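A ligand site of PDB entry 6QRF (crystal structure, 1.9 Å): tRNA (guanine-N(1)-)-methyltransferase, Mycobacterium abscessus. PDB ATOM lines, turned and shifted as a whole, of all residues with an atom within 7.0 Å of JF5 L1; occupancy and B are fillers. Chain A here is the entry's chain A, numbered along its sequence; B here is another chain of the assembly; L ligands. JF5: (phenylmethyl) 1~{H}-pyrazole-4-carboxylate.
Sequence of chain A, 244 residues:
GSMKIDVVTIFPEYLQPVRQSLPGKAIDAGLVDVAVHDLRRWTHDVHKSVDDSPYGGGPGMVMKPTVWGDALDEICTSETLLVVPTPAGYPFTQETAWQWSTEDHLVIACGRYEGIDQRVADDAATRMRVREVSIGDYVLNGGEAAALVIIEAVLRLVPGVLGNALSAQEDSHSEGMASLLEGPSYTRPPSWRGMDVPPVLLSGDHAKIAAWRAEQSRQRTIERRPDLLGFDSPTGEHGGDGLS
Pro 85 touches JF5 L1.
C of Thr 86 touches C04 of JF5 L1, 3.7 Å away.
Pro 87 touches JF5 L1.
CA of Tyr 113 touches C12 of JF5 L1, 3.8 Å away.
Glu 114 touches JF5 L1 (C to C13, 3.7 Å).
CA of Gly 115 touches C13 of JF5 L1, at 3.7 Å.
O of Tyr 138 touches C07 of JF5 L1, 3.0 Å away.
Val 139 touches JF5 L1 (C to O01, 3.9 Å).
Gly 142 touches JF5 L1 (C to C09, 3.3 Å).
Gly 143 touches JF5 L1.
Hydrophobic or aromatic side chains that line JF5 L1: Pro 87, Ile 135 and Leu 140.
Within 4 Å of JF5 L1: Pro 85, Thr 86, Pro 87, Tyr 113, Glu 114, Gly 115, Ser 134, Ile 135, Gly 136, Tyr 138, Val 139, Leu 140, Gly 142 and Gly 143.
The backbone NH (N) of Leu 140 sits at hydrogen-bond distance from an oxygen (O01) of JF5 L1, 2.9 Å away.
A nitrogen (N05) of JF5 L1 sits close to the backbone NH of Ile 135, at 2.9 Å.
N06 of JF5 L1 lies close to O of Gly 136 (3.0 Å).
N06 of JF5 L1 lies within hydrogen-bond range of OG of Ser 134 (3.3 Å).
The side-chain hydroxyl (OH) of Tyr 138 lies within hydrogen-bond range of the backbone carbonyl oxygen (O) of Ile 135 (3.2 Å).
O of Gly 136 lies within hydrogen-bond range of OG of Ser 134 (2.9 Å).
The backbone carbonyl oxygen of Gly 111 lies within hydrogen-bond range of the backbone NH of Gly 143 (2.8 Å).
The backbone NH of Thr 86 sits at hydrogen-bond distance from the backbone carbonyl oxygen of Val 133 (2.9 Å).
N of Ala 88 sits close to OG1 of Thr 86 (3.1 Å).
N of Tyr 113 is in hydrogen-bond range of O of Asn 141 (2.8 Å).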
ATOM      1  N   VAL A  84       4.319 -20.742 -12.180  1.00  0.00           N
ATOM      2  CA  VAL A  84       3.682 -20.965 -10.869  1.00  0.00           C
ATOM      3  C   VAL A  84       2.479 -21.867 -11.031  1.00  0.00           C
ATOM      4  O   VAL A  84       1.436 -21.426 -11.502  1.00  0.00           O
ATOM      5  CB  VAL A  84       3.210 -19.642 -10.227  1.00  0.00           C
ATOM      6  CG1 VAL A  84       2.656 -19.913  -8.821  1.00  0.00           C
ATOM      7  CG2 VAL A  84       4.331 -18.623 -10.194  1.00  0.00           C
ATOM      8  N   PRO A  85       2.620 -23.148 -10.661  1.00  0.00           N
ATOM      9  CA  PRO A  85       1.441 -24.006 -10.813  1.00  0.00           C
ATOM     10  C   PRO A  85       0.382 -23.704  -9.755  1.00  0.00           C
ATOM     11  O   PRO A  85       0.682 -23.513  -8.580  1.00  0.00           O
ATOM     12  CB  PRO A  85       2.006 -25.433 -10.647  1.00  0.00           C
ATOM     13  CG  PRO A  85       3.496 -25.290 -10.874  1.00  0.00           C
ATOM     14  CD  PRO A  85       3.857 -23.909 -10.405  1.00  0.00           C
ATOM     15  N   THR A  86      -0.872 -23.658 -10.181  1.00  0.00           N
ATOM     16  CA  THR A  86      -1.973 -23.385  -9.257  1.00  0.00           C
ATOM     17  C   THR A  86      -3.286 -23.750  -9.961  1.00  0.00           C
ATOM     18  O   THR A  86      -3.401 -23.605 -11.174  1.00  0.00           O
ATOM     19  CB  THR A  86      -2.019 -21.915  -8.836  1.00  0.00           C
ATOM     20  OG1 THR A  86      -3.296 -21.612  -8.264  1.00  0.00           O
ATOM     21  CG2 THR A  86      -1.761 -20.996 -10.006  1.00  0.00           C
ATOM     22  N   PRO A  87      -4.264 -24.235  -9.211  1.00  0.00           N
ATOM     23  CA  PRO A  87      -5.536 -24.586  -9.863  1.00  0.00           C
ATOM     24  C   PRO A  87      -6.274 -23.350 -10.388  1.00  0.00           C
ATOM     25  O   PRO A  87      -7.246 -23.484 -11.113  1.00  0.00           O
ATOM     26  CB  PRO A  87      -6.350 -25.264  -8.742  1.00  0.00           C
ATOM     27  CG  PRO A  87      -5.697 -24.836  -7.471  1.00  0.00           C
ATOM     28  CD  PRO A  87      -4.253 -24.574  -7.781  1.00  0.00           C
ATOM     29  N   ALA A  88      -5.816 -22.168 -10.016  1.00  0.00           N
ATOM     30  CA  ALA A  88      -6.430 -20.936 -10.474  1.00  0.00           C
ATOM     31  C   ALA A  88      -5.709 -20.339 -11.673  1.00  0.00           C
ATOM     32  O   ALA A  88      -5.941 -19.189 -12.036  1.00  0.00           O
ATOM     33  CB  ALA A  88      -6.470 -19.914  -9.327  1.00  0.00           C
ATOM     34  N   GLY A  89      -4.813 -21.117 -12.296  1.00  0.00           N
ATOM     35  CA  GLY A  89      -3.974 -20.589 -13.360  1.00  0.00           C
ATOM     36  C   GLY A  89      -4.625 -20.729 -14.717  1.00  0.00           C
ATOM     37  O   GLY A  89      -5.717 -21.292 -14.844  1.00  0.00           O
ATOM     38  N   ALA A 109       7.894 -22.440  -9.220  1.00  0.00           N
ATOM     39  CA  ALA A 109       7.627 -22.152  -7.819  1.00  0.00           C
ATOM     40  C   ALA A 109       6.443 -22.967  -7.312  1.00  0.00           C
ATOM     41  O   ALA A 109       5.284 -22.695  -7.642  1.00  0.00           O
ATOM     42  CB  ALA A 109       7.375 -20.668  -7.624  1.00  0.00           C
ATOM     43  N   CYS A 110       6.757 -23.977  -6.507  1.00  0.00           N
ATOM     44  CA  CYS A 110       5.758 -24.873  -5.965  1.00  0.00           C
ATOM     45  C   CYS A 110       5.141 -24.304  -4.704  1.00  0.00           C
ATOM     46  O   CYS A 110       5.775 -24.241  -3.661  1.00  0.00           O
ATOM     47  CB  CYS A 110       6.350 -26.243  -5.685  1.00  0.00           C
ATOM     48  SG  CYS A 110       7.088 -27.001  -7.152  1.00  0.00           S
ATOM     49  N   GLY A 111       3.873 -23.918  -4.811  1.00  0.00           N
ATOM     50  CA  GLY A 111       3.125 -23.420  -3.683  1.00  0.00           C
ATOM     51  C   GLY A 111       2.442 -24.553  -2.948  1.00  0.00           C
ATOM     52  O   GLY A 111       2.332 -25.666  -3.460  1.00  0.00           O
ATOM     53  N   ARG A 112       1.997 -24.275  -1.736  1.00  0.00           N
ATOM     54  CA  ARG A 112       1.172 -25.217  -1.022  1.00  0.00           C
ATOM     55  C   ARG A 112      -0.185 -24.626  -0.709  1.00  0.00           C
ATOM     56  O   ARG A 112      -0.306 -23.404  -0.505  1.00  0.00           O
ATOM     57  CB  ARG A 112       1.851 -25.701   0.261  1.00  0.00           C
ATOM     58  CG  ARG A 112       2.924 -26.741  -0.028  1.00  0.00           C
ATOM     59  CD  ARG A 112       2.688 -28.001   0.782  1.00  0.00           C
ATOM     60  NE  ARG A 112       2.978 -29.208  -0.005  1.00  0.00           N
ATOM     61  CZ  ARG A 112       2.487 -30.413   0.253  1.00  0.00           C
ATOM     62  NH1 ARG A 112       1.677 -30.591   1.293  1.00  0.00           N
ATOM     63  NH2 ARG A 112       2.810 -31.438  -0.516  1.00  0.00           N
ATOM     64  N   TYR A 113      -1.173 -25.522  -0.681  1.00  0.00           N
ATOM     65  CA  TYR A 113      -2.599 -25.260  -0.528  1.00  0.00           C
ATOM     66  C   TYR A 113      -2.957 -23.909   0.053  1.00  0.00           C
ATOM     67  O   TYR A 113      -2.490 -23.517   1.125  1.00  0.00           O
ATOM     68  CB  TYR A 113      -3.231 -26.360   0.345  1.00  0.00           C
ATOM     69  N   GLU A 114      -3.862 -23.265  -0.685  1.00  0.00           N
ATOM     70  CA  GLU A 114      -4.245 -21.852  -0.624  1.00  0.00           C
ATOM     71  C   GLU A 114      -3.338 -21.039  -1.541  1.00  0.00           C
ATOM     72  O   GLU A 114      -3.827 -20.288  -2.373  1.00  0.00           O
ATOM     73  CB  GLU A 114      -4.237 -21.300   0.786  1.00  0.00           C
ATOM     74  CG  GLU A 114      -4.595 -19.834   0.871  1.00  0.00           C
ATOM     75  CD  GLU A 114      -5.930 -19.582   1.560  1.00  0.00           C
ATOM     76  OE1 GLU A 114      -6.531 -20.554   2.084  1.00  0.00           O
ATOM     77  OE2 GLU A 114      -6.359 -18.409   1.583  1.00  0.00           O
ATOM     78  N   GLY A 115      -2.017 -21.192  -1.406  1.00  0.00           N
ATOM     79  CA  GLY A 115      -1.116 -20.641  -2.397  1.00  0.00           C
ATOM     80  C   GLY A 115      -0.110 -19.625  -1.880  1.00  0.00           C
ATOM     81  O   GLY A 115       0.105 -19.522  -0.672  1.00  0.00           O
ATOM     82  N   ILE A 116       0.487 -18.880  -2.809  1.00  0.00           N
ATOM     83  CA  ILE A 116       1.511 -17.880  -2.487  1.00  0.00           C
ATOM     84  C   ILE A 116       0.904 -16.476  -2.521  1.00  0.00           C
ATOM     85  O   ILE A 116       0.100 -16.180  -3.407  1.00  0.00           O
ATOM     86  CB  ILE A 116       2.672 -17.962  -3.480  1.00  0.00           C
ATOM     87  CG1 ILE A 116       3.141 -19.416  -3.609  1.00  0.00           C
ATOM     88  CG2 ILE A 116       3.822 -16.973  -3.115  1.00  0.00           C
ATOM     89  CD1 ILE A 116       4.202 -19.639  -4.667  1.00  0.00           C
ATOM     90  N   VAL A 133      -0.194 -21.246 -14.044  1.00  0.00           N
ATOM     91  CA  VAL A 133      -0.868 -22.239 -14.873  1.00  0.00           C
ATOM     92  C   VAL A 133      -1.455 -23.389 -14.074  1.00  0.00           C
ATOM     93  O   VAL A 133      -0.949 -23.774 -13.037  1.00  0.00           O
ATOM     94  CB  VAL A 133       0.082 -22.871 -15.931  1.00  0.00           C
ATOM     95  CG1 VAL A 133       0.502 -21.864 -16.996  1.00  0.00           C
ATOM     96  CG2 VAL A 133       1.273 -23.507 -15.250  1.00  0.00           C
ATOM     97  N   SER A 134      -2.517 -23.961 -14.622  1.00  0.00           N
ATOM     98  CA  SER A 134      -3.161 -25.127 -14.036  1.00  0.00           C
ATOM     99  C   SER A 134      -2.919 -26.336 -14.918  1.00  0.00           C
ATOM    100  O   SER A 134      -3.070 -26.241 -16.136  1.00  0.00           O
ATOM    101  CB  SER A 134      -4.655 -24.907 -13.898  1.00  0.00           C
ATOM    102  OG  SER A 134      -5.283 -26.119 -13.549  1.00  0.00           O
ATOM    103  N   ILE A 135      -2.548 -27.474 -14.336  1.00  0.00           N
ATOM    104  CA  ILE A 135      -2.394 -28.662 -15.179  1.00  0.00           C
ATOM    105  C   ILE A 135      -3.712 -29.455 -15.298  1.00  0.00           C
ATOM    106  O   ILE A 135      -3.757 -30.500 -15.955  1.00  0.00           O
ATOM    107  CB  ILE A 135      -1.299 -29.607 -14.640  1.00  0.00           C
ATOM    108  CG1 ILE A 135      -1.642 -30.058 -13.218  1.00  0.00           C
ATOM    109  CG2 ILE A 135       0.109 -28.950 -14.734  1.00  0.00           C
ATOM    110  CD1 ILE A 135      -0.994 -31.357 -12.820  1.00  0.00           C
ATOM    111  N   GLY A 136      -4.766 -28.976 -14.652  1.00  0.00           N
ATOM    112  CA  GLY A 136      -6.040 -29.678 -14.697  1.00  0.00           C
ATOM    113  C   GLY A 136      -6.971 -29.207 -13.611  1.00  0.00           C
ATOM    114  O   GLY A 136      -6.562 -28.529 -12.669  1.00  0.00           O
ATOM    115  N   ASP A 137      -8.240 -29.576 -13.739  1.00  0.00           N
ATOM    116  CA  ASP A 137      -9.280 -29.070 -12.849  1.00  0.00           C
ATOM    117  C   ASP A 137      -9.496 -29.951 -11.630  1.00  0.00           C
ATOM    118  O   ASP A 137     -10.508 -30.645 -11.511  1.00  0.00           O
ATOM    119  CB  ASP A 137     -10.608 -28.892 -13.607  1.00  0.00           C
ATOM    120  CG  ASP A 137     -10.587 -27.690 -14.512  1.00  0.00           C
ATOM    121  OD1 ASP A 137      -9.797 -26.765 -14.231  1.00  0.00           O
ATOM    122  OD2 ASP A 137     -11.346 -27.663 -15.499  1.00  0.00           O
ATOM    123  N   TYR A 138      -8.533 -29.884 -10.729  1.00  0.00           N
ATOM    124  CA  TYR A 138      -8.566 -30.614  -9.479  1.00  0.00           C
ATOM    125  C   TYR A 138      -7.625 -29.896  -8.517  1.00  0.00           C
ATOM    126  O   TYR A 138      -6.811 -29.067  -8.936  1.00  0.00           O
ATOM    127  CB  TYR A 138      -8.163 -32.082  -9.680  1.00  0.00           C
ATOM    128  CG  TYR A 138      -7.064 -32.234 -10.705  1.00  0.00           C
ATOM    129  CD1 TYR A 138      -5.749 -31.873 -10.396  1.00  0.00           C
ATOM    130  CD2 TYR A 138      -7.330 -32.734 -11.974  1.00  0.00           C
ATOM    131  CE1 TYR A 138      -4.731 -31.983 -11.340  1.00  0.00           C
ATOM    132  CE2 TYR A 138      -6.340 -32.869 -12.913  1.00  0.00           C
ATOM    133  CZ  TYR A 138      -5.038 -32.481 -12.602  1.00  0.00           C
ATOM    134  OH  TYR A 138      -4.045 -32.592 -13.544  1.00  0.00           O
ATOM    135  N   VAL A 139      -7.736 -30.222  -7.239  1.00  0.00           N
ATOM    136  CA  VAL A 139      -6.914 -29.542  -6.243  1.00  0.00           C
ATOM    137  C   VAL A 139      -5.921 -30.508  -5.649  1.00  0.00           C
ATOM    138  O   VAL A 139      -6.270 -31.614  -5.257  1.00  0.00           O
ATOM    139  CB  VAL A 139      -7.775 -28.932  -5.104  1.00  0.00           C
ATOM    140  CG1 VAL A 139      -6.870 -28.237  -4.074  1.00  0.00           C
ATOM    141  CG2 VAL A 139      -8.783 -27.964  -5.671  1.00  0.00           C
ATOM    142  N   LEU A 140      -4.652 -30.097  -5.608  1.00  0.00           N
ATOM    143  CA  LEU A 140      -3.616 -30.890  -4.983  1.00  0.00           C
ATOM    144  C   LEU A 140      -3.231 -30.191  -3.692  1.00  0.00           C
ATOM    145  O   LEU A 140      -3.609 -29.035  -3.491  1.00  0.00           O
ATOM    146  CB  LEU A 140      -2.391 -31.037  -5.905  1.00  0.00           C
ATOM    147  CG  LEU A 140      -2.713 -31.457  -7.350  1.00  0.00           C
ATOM    148  CD1 LEU A 140      -1.459 -31.543  -8.189  1.00  0.00           C
ATOM    149  CD2 LEU A 140      -3.464 -32.790  -7.377  1.00  0.00           C
ATOM    150  N   ASN A 141      -2.445 -30.847  -2.846  1.00  0.00           N
ATOM    151  CA  ASN A 141      -1.993 -30.211  -1.614  1.00  0.00           C
ATOM    152  C   ASN A 141      -0.850 -29.238  -1.905  1.00  0.00           C
ATOM    153  O   ASN A 141      -0.624 -28.271  -1.160  1.00  0.00           O
ATOM    154  CB  ASN A 141      -1.532 -31.260  -0.610  1.00  0.00           C
ATOM    155  CG  ASN A 141      -2.600 -31.561   0.433  1.00  0.00           C
ATOM    156  OD1 ASN A 141      -3.511 -30.760   0.648  1.00  0.00           O
ATOM    157  ND2 ASN A 141      -2.486 -32.707   1.083  1.00  0.00           N
ATOM    158  N   GLY A 142      -0.122 -29.483  -2.992  1.00  0.00           N
ATOM    159  CA  GLY A 142       1.025 -28.658  -3.334  1.00  0.00           C
ATOM    160  C   GLY A 142       1.371 -28.746  -4.804  1.00  0.00           C
ATOM    161  O   GLY A 142       0.896 -29.634  -5.521  1.00  0.00           O
ATOM    162  N   GLY A 143       2.220 -27.818  -5.260  1.00  0.00           N
ATOM    163  CA  GLY A 143       2.550 -27.742  -6.669  1.00  0.00           C
ATOM    164  C   GLY A 143       3.515 -28.798  -7.189  1.00  0.00           C
ATOM    165  O   GLY A 143       3.739 -28.883  -8.384  1.00  0.00           O
ATOM    166  N   GLU A 144       4.061 -29.619  -6.290  1.00  0.00           N
ATOM    167  CA  GLU A 144       5.142 -30.511  -6.677  1.00  0.00           C
ATOM    168  C   GLU A 144       4.748 -31.549  -7.724  1.00  0.00           C
ATOM    169  O   GLU A 144       5.514 -31.805  -8.635  1.00  0.00           O
ATOM    170  CB  GLU A 144       5.706 -31.234  -5.436  1.00  0.00           C
ATOM    171  CG  GLU A 144       6.572 -30.335  -4.529  1.00  0.00           C
ATOM    172  CD  GLU A 144       5.749 -29.463  -3.601  1.00  0.00           C
ATOM    173  OE1 GLU A 144       4.526 -29.666  -3.502  1.00  0.00           O
ATOM    174  OE2 GLU A 144       6.333 -28.586  -2.925  1.00  0.00           O
ATOM    175  N   ALA A 146       2.438 -31.150  -9.916  1.00  0.00           N
ATOM    176  CA  ALA A 146       2.210 -30.380 -11.131  1.00  0.00           C
ATOM    177  C   ALA A 146       3.535 -30.006 -11.784  1.00  0.00           C
ATOM    178  O   ALA A 146       3.639 -30.001 -13.010  1.00  0.00           O
ATOM    179  CB  ALA A 146       1.370 -29.130 -10.842  1.00  0.00           C
ATOM    180  N   GLU B 152      -2.741 -37.873  -5.154  1.00  0.00           N
ATOM    181  CA  GLU B 152      -2.819 -36.670  -4.335  1.00  0.00           C
ATOM    182  C   GLU B 152      -4.224 -36.093  -4.329  1.00  0.00           C
ATOM    183  O   GLU B 152      -4.756 -35.762  -3.278  1.00  0.00           O
ATOM    184  CB  GLU B 152      -1.846 -35.579  -4.821  1.00  0.00           C
ATOM    185  CG  GLU B 152      -0.460 -35.690  -4.243  1.00  0.00           C
ATOM    186  CD  GLU B 152       0.214 -34.328  -4.082  1.00  0.00           C
ATOM    187  OE1 GLU B 152       1.434 -34.262  -4.275  1.00  0.00           O
ATOM    188  OE2 GLU B 152      -0.481 -33.336  -3.745  1.00  0.00           O
HETATM  189  C10 JF5 L   1      -1.653 -25.514  -5.466  1.00  0.00           C
HETATM  190  C13 JF5 L   1      -2.831 -23.232  -4.435  1.00  0.00           C
HETATM  191  C15 JF5 L   1      -1.097 -24.268  -5.722  1.00  0.00           C
HETATM  192  O01 JF5 L   1      -3.147 -28.078  -6.953  1.00  0.00           O
HETATM  193  C02 JF5 L   1      -2.464 -27.556  -7.813  1.00  0.00           C
HETATM  194  C03 JF5 L   1      -2.860 -27.629  -9.288  1.00  0.00           C
HETATM  195  C04 JF5 L   1      -2.100 -27.184 -10.338  1.00  0.00           C
HETATM  196  N05 JF5 L   1      -2.795 -27.415 -11.450  1.00  0.00           N
HETATM  197  N06 JF5 L   1      -3.999 -27.961 -11.163  1.00  0.00           N
HETATM  198  C07 JF5 L   1      -4.053 -28.122  -9.807  1.00  0.00           C
HETATM  199  O08 JF5 L   1      -1.282 -26.851  -7.459  1.00  0.00           O
HETATM  200  C09 JF5 L   1      -1.013 -26.776  -6.041  1.00  0.00           C
HETATM  201  C11 JF5 L   1      -2.807 -25.620  -4.688  1.00  0.00           C
HETATM  202  C12 JF5 L   1      -3.378 -24.475  -4.175  1.00  0.00           C
HETATM  203  C14 JF5 L   1      -1.684 -23.120  -5.204  1.00  0.00           C
HETATM  204  C10 JF5 L   2     -10.470 -25.301  -9.519  1.00  0.00           C
HETATM  205  C13 JF5 L   2     -11.714 -27.620 -10.362  1.00  0.00           C
HETATM  206  C15 JF5 L   2     -11.143 -25.320 -10.741  1.00  0.00           C
HETATM  207  O01 JF5 L   2      -8.817 -21.918  -7.683  1.00  0.00           O
HETATM  208  C02 JF5 L   2      -8.911 -22.968  -7.082  1.00  0.00           C
HETATM  209  C03 JF5 L   2      -8.246 -23.145  -5.720  1.00  0.00           C
HETATM  210  C04 JF5 L   2      -7.117 -22.496  -5.280  1.00  0.00           C
HETATM  211  N05 JF5 L   2      -6.880 -22.931  -4.036  1.00  0.00           N
HETATM  212  N06 JF5 L   2      -7.818 -23.837  -3.662  1.00  0.00           N
HETATM  213  C07 JF5 L   2      -8.682 -23.989  -4.693  1.00  0.00           C
HETATM  214  O08 JF5 L   2      -9.659 -24.048  -7.632  1.00  0.00           O
HETATM  215  C09 JF5 L   2      -9.792 -24.012  -9.058  1.00  0.00           C
HETATM  216  C11 JF5 L   2     -10.425 -26.436  -8.737  1.00  0.00           C
HETATM  217  C12 JF5 L   2     -11.046 -27.602  -9.154  1.00  0.00           C
HETATM  218  C14 JF5 L   2     -11.769 -26.477 -11.157  1.00  0.00           C
